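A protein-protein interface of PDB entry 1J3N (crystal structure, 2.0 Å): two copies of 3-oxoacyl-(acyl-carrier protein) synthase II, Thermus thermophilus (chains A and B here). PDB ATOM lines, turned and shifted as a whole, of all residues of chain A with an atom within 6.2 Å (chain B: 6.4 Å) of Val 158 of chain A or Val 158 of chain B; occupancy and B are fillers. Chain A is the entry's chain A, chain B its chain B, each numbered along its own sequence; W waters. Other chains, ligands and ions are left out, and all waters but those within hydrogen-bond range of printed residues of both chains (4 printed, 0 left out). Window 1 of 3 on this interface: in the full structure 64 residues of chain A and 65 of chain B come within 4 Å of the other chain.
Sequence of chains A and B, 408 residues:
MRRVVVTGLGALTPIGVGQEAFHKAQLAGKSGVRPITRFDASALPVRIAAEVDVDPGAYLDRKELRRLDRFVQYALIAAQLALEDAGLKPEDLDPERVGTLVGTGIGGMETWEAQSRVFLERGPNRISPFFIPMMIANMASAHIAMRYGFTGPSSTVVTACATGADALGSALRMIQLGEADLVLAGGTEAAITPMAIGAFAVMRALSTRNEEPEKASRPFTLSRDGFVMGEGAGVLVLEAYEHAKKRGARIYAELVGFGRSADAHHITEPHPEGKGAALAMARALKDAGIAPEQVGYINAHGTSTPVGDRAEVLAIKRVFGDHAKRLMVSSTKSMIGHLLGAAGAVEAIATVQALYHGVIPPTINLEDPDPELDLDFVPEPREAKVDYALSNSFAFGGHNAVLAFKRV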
ATOM      1  N   GLY A 103      21.622  -9.701   5.905  1.00  0.00           N
ATOM      2  CA  GLY A 103      20.192  -9.892   5.765  1.00  0.00           C
ATOM      3  C   GLY A 103      19.462  -9.818   7.090  1.00  0.00           C
ATOM      4  O   GLY A 103      20.078  -9.666   8.147  1.00  0.00           O
ATOM      5  N   THR A 104      18.140  -9.910   7.022  1.00  0.00           N
ATOM      6  CA  THR A 104      17.295  -9.880   8.210  1.00  0.00           C
ATOM      7  C   THR A 104      16.016 -10.613   7.823  1.00  0.00           C
ATOM      8  O   THR A 104      15.706 -10.732   6.646  1.00  0.00           O
ATOM      9  CB  THR A 104      16.966  -8.426   8.621  1.00  0.00           C
ATOM     10  OG1 THR A 104      16.171  -8.431   9.806  1.00  0.00           O
ATOM     11  CG2 THR A 104      16.212  -7.717   7.504  1.00  0.00           C
ATOM     12  N   GLY A 105      15.279 -11.123   8.801  1.00  0.00           N
ATOM     13  CA  GLY A 105      14.054 -11.827   8.475  1.00  0.00           C
ATOM     14  C   GLY A 105      12.821 -10.940   8.512  1.00  0.00           C
ATOM     15  O   GLY A 105      11.923 -11.073   7.668  1.00  0.00           O
ATOM     16  N   ILE A 106      12.790 -10.021   9.477  1.00  0.00           N
ATOM     17  CA  ILE A 106      11.654  -9.123   9.681  1.00  0.00           C
ATOM     18  C   ILE A 106      11.968  -7.634   9.484  1.00  0.00           C
ATOM     19  O   ILE A 106      11.100  -6.862   9.073  1.00  0.00           O
ATOM     20  CB  ILE A 106      11.090  -9.324  11.114  1.00  0.00           C
ATOM     21  CG1 ILE A 106      10.516 -10.736  11.246  1.00  0.00           C
ATOM     22  CG2 ILE A 106      10.034  -8.276  11.435  1.00  0.00           C
ATOM     23  CD1 ILE A 106       9.852 -10.999  12.583  1.00  0.00           C
ATOM     24  N   ILE A 136      12.760  -0.819   6.429  1.00  0.00           N
ATOM     25  CA  ILE A 136      13.067  -1.764   5.355  1.00  0.00           C
ATOM     26  C   ILE A 136      14.357  -2.571   5.527  1.00  0.00           C
ATOM     27  O   ILE A 136      15.376  -2.065   5.989  1.00  0.00           O
ATOM     28  CB  ILE A 136      13.034  -1.075   3.962  1.00  0.00           C
ATOM     29  CG1 ILE A 136      14.046   0.063   3.881  1.00  0.00           C
ATOM     30  CG2 ILE A 136      11.635  -0.513   3.705  1.00  0.00           C
ATOM     31  CD1 ILE A 136      14.072   0.733   2.516  1.00  0.00           C
ATOM     32  N   ALA A 137      14.284  -3.841   5.137  1.00  0.00           N
ATOM     33  CA  ALA A 137      15.382  -4.804   5.276  1.00  0.00           C
ATOM     34  C   ALA A 137      16.756  -4.437   4.748  1.00  0.00           C
ATOM     35  O   ALA A 137      17.760  -4.783   5.363  1.00  0.00           O
ATOM     36  CB  ALA A 137      14.957  -6.159   4.671  1.00  0.00           C
ATOM     37  N   ASN A 138      16.806  -3.752   3.613  1.00  0.00           N
ATOM     38  CA  ASN A 138      18.077  -3.388   3.002  1.00  0.00           C
ATOM     39  C   ASN A 138      18.848  -2.289   3.725  1.00  0.00           C
ATOM     40  O   ASN A 138      19.942  -1.919   3.294  1.00  0.00           O
ATOM     41  CB  ASN A 138      17.836  -2.962   1.554  1.00  0.00           C
ATOM     42  CG  ASN A 138      16.912  -1.753   1.451  1.00  0.00           C
ATOM     43  OD1 ASN A 138      17.350  -0.638   1.155  1.00  0.00           O
ATOM     44  ND2 ASN A 138      15.630  -1.970   1.711  1.00  0.00           N
ATOM     45  N   SER A 155      23.825  -5.803  -1.198  1.00  0.00           N
ATOM     46  CA  SER A 155      22.550  -6.504  -1.315  1.00  0.00           C
ATOM     47  C   SER A 155      21.992  -7.013   0.006  1.00  0.00           C
ATOM     48  O   SER A 155      22.656  -6.970   1.046  1.00  0.00           O
ATOM     49  CB  SER A 155      22.671  -7.663  -2.311  1.00  0.00           C
ATOM     50  OG  SER A 155      21.381  -8.075  -2.751  1.00  0.00           O
ATOM     51  N   THR A 156      20.754  -7.497  -0.053  1.00  0.00           N
ATOM     52  CA  THR A 156      20.055  -7.991   1.120  1.00  0.00           C
ATOM     53  C   THR A 156      19.140  -9.165   0.798  1.00  0.00           C
ATOM     54  O   THR A 156      18.326  -9.086  -0.113  1.00  0.00           O
ATOM     55  CB  THR A 156      19.176  -6.873   1.738  1.00  0.00           C
ATOM     56  OG1 THR A 156      20.000  -5.772   2.149  1.00  0.00           O
ATOM     57  CG2 THR A 156      18.394  -7.410   2.928  1.00  0.00           C
ATOM     58  N   VAL A 157      19.274 -10.250   1.554  1.00  0.00           N
ATOM     59  CA  VAL A 157      18.419 -11.417   1.369  1.00  0.00           C
ATOM     60  C   VAL A 157      17.539 -11.557   2.613  1.00  0.00           C
ATOM     61  O   VAL A 157      17.969 -11.263   3.736  1.00  0.00           O
ATOM     62  CB  VAL A 157      19.244 -12.718   1.180  1.00  0.00           C
ATOM     63  CG1 VAL A 157      20.066 -12.640  -0.101  1.00  0.00           C
ATOM     64  CG2 VAL A 157      20.150 -12.939   2.379  1.00  0.00           C
ATOM     65  N   VAL A 158      16.299 -11.976   2.394  1.00  0.00           N
ATOM     66  CA  VAL A 158      15.329 -12.173   3.455  1.00  0.00           C
ATOM     67  C   VAL A 158      14.697 -13.538   3.216  1.00  0.00           C
ATOM     68  O   VAL A 158      13.823 -13.682   2.362  1.00  0.00           O
ATOM     69  CB  VAL A 158      14.222 -11.081   3.420  1.00  0.00           C
ATOM     70  CG1 VAL A 158      13.177 -11.348   4.506  1.00  0.00           C
ATOM     71  CG2 VAL A 158      14.854  -9.698   3.625  1.00  0.00           C
ATOM     72  N   THR A 159      15.172 -14.538   3.950  1.00  0.00           N
ATOM     73  CA  THR A 159      14.654 -15.888   3.831  1.00  0.00           C
ATOM     74  C   THR A 159      14.433 -16.501   5.212  1.00  0.00           C
ATOM     75  O   THR A 159      14.807 -17.645   5.486  1.00  0.00           O
ATOM     76  CB  THR A 159      15.600 -16.774   2.987  1.00  0.00           C
ATOM     77  OG1 THR A 159      16.950 -16.626   3.443  1.00  0.00           O
ATOM     78  CG2 THR A 159      15.519 -16.376   1.512  1.00  0.00           C
ATOM     79  N   ALA A 160      13.815 -15.712   6.083  1.00  0.00           N
ATOM     80  CA  ALA A 160      13.522 -16.149   7.434  1.00  0.00           C
ATOM     81  C   ALA A 160      14.737 -16.794   8.110  1.00  0.00           C
ATOM     82  O   ALA A 160      15.811 -16.198   8.189  1.00  0.00           O
ATOM     83  CB  ALA A 160      12.337 -17.120   7.410  1.00  0.00           C
ATOM     84  N   THR A 163      18.176 -16.947   6.303  1.00  0.00           N
ATOM     85  CA  THR A 163      18.773 -15.652   5.976  1.00  0.00           C
ATOM     86  C   THR A 163      20.292 -15.561   6.169  1.00  0.00           C
ATOM     87  O   THR A 163      21.039 -15.278   5.233  1.00  0.00           O
ATOM     88  CB  THR A 163      18.118 -14.525   6.819  1.00  0.00           C
ATOM     89  OG1 THR A 163      16.694 -14.557   6.645  1.00  0.00           O
ATOM     90  CG2 THR A 163      18.638 -13.163   6.394  1.00  0.00           C
ATOM     91  N   ASP A 166      22.168 -17.928   3.773  1.00  0.00           N
ATOM     92  CA  ASP A 166      21.885 -17.534   2.399  1.00  0.00           C
ATOM     93  C   ASP A 166      22.747 -16.296   2.092  1.00  0.00           C
ATOM     94  O   ASP A 166      23.367 -16.193   1.027  1.00  0.00           O
ATOM     95  CB  ASP A 166      20.390 -17.188   2.284  1.00  0.00           C
ATOM     96  CG  ASP A 166      19.837 -17.353   0.874  1.00  0.00           C
ATOM     97  OD1 ASP A 166      20.616 -17.384  -0.102  1.00  0.00           O
ATOM     98  OD2 ASP A 166      18.595 -17.430   0.746  1.00  0.00           O
ATOM     99  N   HIS A 399      12.742 -22.726   2.789  1.00  0.00           N
ATOM    100  CA  HIS A 399      14.080 -22.347   2.352  1.00  0.00           C
ATOM    101  C   HIS A 399      15.145 -23.077   3.169  1.00  0.00           C
ATOM    102  O   HIS A 399      15.199 -22.947   4.394  1.00  0.00           O
ATOM    103  CB  HIS A 399      14.262 -20.836   2.505  1.00  0.00           C
ATOM    104  CG  HIS A 399      13.080 -20.048   2.053  1.00  0.00           C
ATOM    105  ND1 HIS A 399      12.923 -19.615   0.753  1.00  0.00           N
ATOM    106  CD2 HIS A 399      11.966 -19.660   2.717  1.00  0.00           C
ATOM    107  CE1 HIS A 399      11.762 -18.994   0.637  1.00  0.00           C
ATOM    108  NE2 HIS A 399      11.162 -19.010   1.815  1.00  0.00           N
ATOM    109  N   GLY B 103      11.827 -11.256  -5.621  1.00  0.00           N
ATOM    110  CA  GLY B 103      11.977 -10.337  -4.517  1.00  0.00           C
ATOM    111  C   GLY B 103      10.796  -9.411  -4.358  1.00  0.00           C
ATOM    112  O   GLY B 103       9.826  -9.475  -5.113  1.00  0.00           O
ATOM    113  N   THR B 104      10.892  -8.556  -3.352  1.00  0.00           N
ATOM    114  CA  THR B 104       9.881  -7.556  -3.042  1.00  0.00           C
ATOM    115  C   THR B 104      10.601  -6.552  -2.147  1.00  0.00           C
ATOM    116  O   THR B 104      11.571  -6.904  -1.474  1.00  0.00           O
ATOM    117  CB  THR B 104       8.676  -8.176  -2.289  1.00  0.00           C
ATOM    118  OG1 THR B 104       7.698  -7.161  -2.029  1.00  0.00           O
ATOM    119  CG2 THR B 104       9.124  -8.806  -0.968  1.00  0.00           C
ATOM    120  N   GLY B 105      10.160  -5.301  -2.152  1.00  0.00           N
ATOM    121  CA  GLY B 105      10.823  -4.317  -1.315  1.00  0.00           C
ATOM    122  C   GLY B 105      10.182  -4.154   0.055  1.00  0.00           C
ATOM    123  O   GLY B 105      10.841  -3.725   1.007  1.00  0.00           O
ATOM    124  N   ILE B 106       8.905  -4.514   0.163  1.00  0.00           N
ATOM    125  CA  ILE B 106       8.180  -4.375   1.424  1.00  0.00           C
ATOM    126  C   ILE B 106       7.421  -5.622   1.870  1.00  0.00           C
ATOM    127  O   ILE B 106       7.208  -5.829   3.064  1.00  0.00           O
ATOM    128  CB  ILE B 106       7.177  -3.199   1.344  1.00  0.00           C
ATOM    129  CG1 ILE B 106       7.935  -1.897   1.086  1.00  0.00           C
ATOM    130  CG2 ILE B 106       6.374  -3.100   2.640  1.00  0.00           C
ATOM    131  CD1 ILE B 106       7.035  -0.717   0.811  1.00  0.00           C
ATOM    132  N   ILE B 136       5.951 -11.989   5.687  1.00  0.00           N
ATOM    133  CA  ILE B 136       7.384 -12.064   5.419  1.00  0.00           C
ATOM    134  C   ILE B 136       7.750 -12.129   3.934  1.00  0.00           C
ATOM    135  O   ILE B 136       7.225 -12.939   3.163  1.00  0.00           O
ATOM    136  CB  ILE B 136       8.077 -13.215   6.209  1.00  0.00           C
ATOM    137  CG1 ILE B 136       7.372 -14.553   5.988  1.00  0.00           C
ATOM    138  CG2 ILE B 136       8.084 -12.877   7.684  1.00  0.00           C
ATOM    139  CD1 ILE B 136       8.039 -15.704   6.755  1.00  0.00           C
ATOM    140  N   ALA B 137       8.667 -11.243   3.564  1.00  0.00           N
ATOM    141  CA  ALA B 137       9.159 -11.070   2.198  1.00  0.00           C
ATOM    142  C   ALA B 137       9.430 -12.322   1.358  1.00  0.00           C
ATOM    143  O   ALA B 137       9.171 -12.330   0.156  1.00  0.00           O
ATOM    144  CB  ALA B 137      10.412 -10.215   2.240  1.00  0.00           C
ATOM    145  N   ASN B 138       9.959 -13.363   1.991  1.00  0.00           N
ATOM    146  CA  ASN B 138      10.315 -14.606   1.303  1.00  0.00           C
ATOM    147  C   ASN B 138       9.167 -15.495   0.839  1.00  0.00           C
ATOM    148  O   ASN B 138       9.393 -16.490   0.135  1.00  0.00           O
ATOM    149  CB  ASN B 138      11.227 -15.441   2.209  1.00  0.00           C
ATOM    150  CG  ASN B 138      10.589 -15.726   3.561  1.00  0.00           C
ATOM    151  OD1 ASN B 138      10.378 -14.812   4.361  1.00  0.00           O
ATOM    152  ND2 ASN B 138      10.262 -16.995   3.816  1.00  0.00           N
ATOM    153  N   MET B 139       7.942 -15.153   1.216  1.00  0.00           N
ATOM    154  CA  MET B 139       6.794 -15.983   0.852  1.00  0.00           C
ATOM    155  C   MET B 139       6.384 -15.973  -0.618  1.00  0.00           C
ATOM    156  O   MET B 139       5.633 -16.850  -1.054  1.00  0.00           O
ATOM    157  CB  MET B 139       5.602 -15.648   1.748  1.00  0.00           C
ATOM    158  CG  MET B 139       5.858 -15.959   3.229  1.00  0.00           C
ATOM    159  SD  MET B 139       6.488 -17.640   3.525  1.00  0.00           S
ATOM    160  CE  MET B 139       5.025 -18.588   3.206  1.00  0.00           C
ATOM    161  N   SER B 155      15.375 -18.397  -3.026  1.00  0.00           N
ATOM    162  CA  SER B 155      15.864 -17.242  -2.297  1.00  0.00           C
ATOM    163  C   SER B 155      15.032 -15.998  -2.570  1.00  0.00           C
ATOM    164  O   SER B 155      14.149 -15.991  -3.430  1.00  0.00           O
ATOM    165  CB  SER B 155      17.339 -16.974  -2.624  1.00  0.00           C
ATOM    166  OG  SER B 155      17.926 -16.139  -1.631  1.00  0.00           O
ATOM    167  N   THR B 156      15.330 -14.942  -1.830  1.00  0.00           N
ATOM    168  CA  THR B 156      14.587 -13.696  -1.935  1.00  0.00           C
ATOM    169  C   THR B 156      15.516 -12.532  -1.669  1.00  0.00           C
ATOM    170  O   THR B 156      16.289 -12.557  -0.715  1.00  0.00           O
ATOM    171  CB  THR B 156      13.469 -13.633  -0.871  1.00  0.00           C
ATOM    172  OG1 THR B 156      12.583 -14.741  -1.041  1.00  0.00           O
ATOM    173  CG2 THR B 156      12.686 -12.318  -0.970  1.00  0.00           C
ATOM    174  N   VAL B 157      15.440 -11.517  -2.519  1.00  0.00           N
ATOM    175  CA  VAL B 157      16.247 -10.321  -2.332  1.00  0.00           C
ATOM    176  C   VAL B 157      15.272  -9.190  -2.007  1.00  0.00           C
ATOM    177  O   VAL B 157      14.149  -9.160  -2.513  1.00  0.00           O
ATOM    178  CB  VAL B 157      17.054  -9.956  -3.604  1.00  0.00           C
ATOM    179  CG1 VAL B 157      18.175 -10.964  -3.828  1.00  0.00           C
ATOM    180  CG2 VAL B 157      16.135  -9.928  -4.806  1.00  0.00           C
ATOM    181  N   VAL B 158      15.706  -8.282  -1.142  1.00  0.00           N
ATOM    182  CA  VAL B 158      14.910  -7.133  -0.729  1.00  0.00           C
ATOM    183  C   VAL B 158      15.872  -5.946  -0.722  1.00  0.00           C
ATOM    184  O   VAL B 158      16.559  -5.705   0.271  1.00  0.00           O
ATOM    185  CB  VAL B 158      14.343  -7.325   0.710  1.00  0.00           C
ATOM    186  CG1 VAL B 158      13.552  -6.095   1.119  1.00  0.00           C
ATOM    187  CG2 VAL B 158      13.466  -8.571   0.776  1.00  0.00           C
ATOM    188  N   THR B 159      15.941  -5.224  -1.835  1.00  0.00           N
ATOM    189  CA  THR B 159      16.836  -4.078  -1.935  1.00  0.00           C
ATOM    190  C   THR B 159      16.143  -2.877  -2.560  1.00  0.00           C
ATOM    191  O   THR B 159      16.650  -2.285  -3.512  1.00  0.00           O
ATOM    192  CB  THR B 159      18.102  -4.407  -2.774  1.00  0.00           C
ATOM    193  OG1 THR B 159      17.719  -5.049  -3.997  1.00  0.00           O
ATOM    194  CG2 THR B 159      19.047  -5.320  -1.995  1.00  0.00           C
ATOM    195  N   ALA B 160      14.978  -2.527  -2.022  1.00  0.00           N
ATOM    196  CA  ALA B 160      14.216  -1.390  -2.513  1.00  0.00           C
ATOM    197  C   ALA B 160      13.976  -1.444  -4.026  1.00  0.00           C
ATOM    198  O   ALA B 160      13.617  -2.493  -4.574  1.00  0.00           O
ATOM    199  CB  ALA B 160      14.935  -0.086  -2.136  1.00  0.00           C
ATOM    200  N   THR B 163      15.503  -4.159  -6.237  1.00  0.00           N
ATOM    201  CA  THR B 163      15.038  -5.529  -6.033  1.00  0.00           C
ATOM    202  C   THR B 163      14.842  -6.364  -7.286  1.00  0.00           C
ATOM    203  O   THR B 163      15.340  -7.486  -7.359  1.00  0.00           O
ATOM    204  CB  THR B 163      13.724  -5.561  -5.229  1.00  0.00           C
ATOM    205  OG1 THR B 163      13.948  -5.006  -3.928  1.00  0.00           O
ATOM    206  CG2 THR B 163      13.226  -7.001  -5.075  1.00  0.00           C
ATOM    207  N   HIS B 399      21.456   1.421  -3.185  1.00  0.00           N
ATOM    208  CA  HIS B 399      21.704   0.154  -3.876  1.00  0.00           C
ATOM    209  C   HIS B 399      21.522   0.370  -5.380  1.00  0.00           C
ATOM    210  O   HIS B 399      20.459   0.802  -5.821  1.00  0.00           O
ATOM    211  CB  HIS B 399      20.710  -0.921  -3.409  1.00  0.00           C
ATOM    212  CG  HIS B 399      20.581  -1.023  -1.922  1.00  0.00           C
ATOM    213  ND1 HIS B 399      21.386  -1.842  -1.156  1.00  0.00           N
ATOM    214  CD2 HIS B 399      19.772  -0.373  -1.053  1.00  0.00           C
ATOM    215  CE1 HIS B 399      21.078  -1.688   0.120  1.00  0.00           C
ATOM    216  NE2 HIS B 399      20.103  -0.801   0.210  1.00  0.00           N
HETATM  217  O   HOH W   1      10.063  -9.847   5.898  1.00  0.00           O
HETATM  218  O   HOH W   2      13.238  -2.650   0.166  1.00  0.00           O
HETATM  219  O   HOH W   3      11.610  -4.652   3.895  1.00  0.00           O
HETATM  220  O   HOH W   4      12.137 -13.640   6.420  1.00  0.00           O
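Among the printed residues, pairs that only touch across the chains: Ala 137 of chain A with Val 158 of chain B, Asn 138 of chain A with Val 158 of chain B, Asn 138 of chain A with Thr 159 of chain B, Asn 138 of chain A with Ala 160 of chain B, Ser 155 of chain A with Thr 159 of chain B, Thr 156 of chain A with Val 157 of chain B, Thr 156 of chain A with Thr 159 of chain B, Val 157 of chain A with Thr 156 of chain B, Val 158 of chain A with Ala 137 of chain B, Val 158 of chain A with Asn 138 of chain B, Val 158 of chain A with Val 158 of chain B, Thr 159 of chain A with Asn 138 of chain B, Thr 159 of chain A with Ser 155 of chain B, Thr 159 of chain A with Thr 156 of chain B and Ala 160 of chain A with Asn 138 of chain B.
The backbone NH (N) of Thr 104 of chain B is in hydrogen-bond range of the backbone carbonyl oxygen (O) of Val 157 of chain B, 3.4 Å away. The side-chain hydroxyl of Thr 159 of chain A is in hydrogen-bond range of the side-chain carboxylate of Asp 166 of chain A (3.3 Å). N of Thr 159 of chain B sits at hydrogen-bond distance from OG1 of Thr 163 of chain B, at 2.9 Å. O of Ala 160 of chain A sits at hydrogen-bond distance from OG1 of Thr 163 of chain A (2.4 Å). The backbone carbonyl oxygen (O) of Ala 160 of chain B lies within hydrogen-bond range of the side-chain hydroxyl (OG1) of Thr 163 of chain B (2.6 Å). The backbone NH of Thr 159 of chain A is in hydrogen-bond range of the side-chain hydroxyl of Thr 163 of chain A (3.1 Å).
Printed residues of chain A that touch a printed residue of chain B: Ala 137, Asn 138, Ser 155, Thr 156, Val 157, Val 158, Thr 159, Ala 160, Asp 166 and His 399. Printed residues of chain B that touch a printed residue of chain A: Ala 137, Asn 138, Ser 155, Thr 156, Val 157, Val 158, Thr 159, Ala 160 and His 399. Hydrophobic or aromatic side chains of chain B within 4 Å of the printed part of chain A: Ala 137, Val 157, Val 158 and His 399. Among the printed residues, 20 pairs touch across the chains. Among the printed residues, no Asp or Glu carboxylate lies within 4 Å of a Lys or Arg side-chain nitrogen of the other chain.
Of the printed residues of chain B, Asn 138 of chain A touches Val 158, Thr 159, Ala 160 and His 399. Val 158 of chain A touches four residues of chain B. Of the printed residues of chain B, Thr 159 of chain A touches Asn 138, Ser 155 and Thr 156. Thr 163 of chain A touches none of the printed residues of chain B. Of the printed residues of chain B, His 399 of chain A touches Asn 138 (3.0 Å). Printed residues of chain A within 4 Å of Ala 137 of chain B: Val 158. Val 158 of chain B touches just these residues of chain A: Ala 137, Asn 138, Thr 156 and Val 158. The nearest residue of chain B that does not touch Val 158 of chain A is Val 157 of chain B (5.0 Å). The nearest printed residue of chain A that does not touch Ser 155 of chain B is Val 157 of chain A (4.4 Å).
Asn 138 of chain A touches Thr 159 of chain B, and with the chains exchanged Thr 159 of chain A touches Asn 138 of chain B. Asn 138 of chain A touches His 399 of chain B, and with the chains exchanged His 399 of chain A touches Asn 138 of chain B. Thr 156 of chain A touches Thr 159 of chain B, and with the chains exchanged Thr 159 of chain A touches Thr 156 of chain B. Val 158 of chain A touches its own counterpart, Val 158 of chain B. 15 positions are printed for both chains.
The backbone NH (N) of Val 158 of chain A sits at hydrogen-bond distance from the backbone carbonyl oxygen (O) of Thr 156 of chain B (3.2 Å). A ring nitrogen (NE2) of His 399 of chain B lies within hydrogen-bond range of the side-chain amide oxygen of Asn 138 of chain A, 2.9 Å away. The side-chain amide nitrogen (ND2) of Asn 138 of chain B sits at hydrogen-bond distance from a ring nitrogen (NE2) of His 399 of chain A (3.0 Å). The backbone carbonyl oxygen (O) of Thr 156 of chain A lies within hydrogen-bond range of the backbone NH (N) of Val 158 of chain B (2.9 Å). The side-chain hydroxyl (OG) of Ser 155 of chain B lies within hydrogen-bond range of the side-chain carboxylate (OD2) of Asp 166 of chain A (2.8 Å).
Water W4 lies within hydrogen-bond range of N of Ala 160 of chain A (2.7 Å), O of Gly 105 of chain A (2.9 Å) and OD1 of Asn 138 of chain B (3.0 Å). Water W2 lies within hydrogen-bond range of O of Gly 105 of chain B, N of Ala 160 of chain B and ND2 of Asn 138 of chain A. Water W1 lies within hydrogen-bond range of O of Gly 105 of chain A (2.8 Å) and N of Ala 137 of chain B (3.1 Å). Water W3 lies within hydrogen-bond range of the backbone NH of Ala 137 of chain A (3.1 Å) and the backbone carbonyl oxygen of Gly 105 of chain B (3.1 Å).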
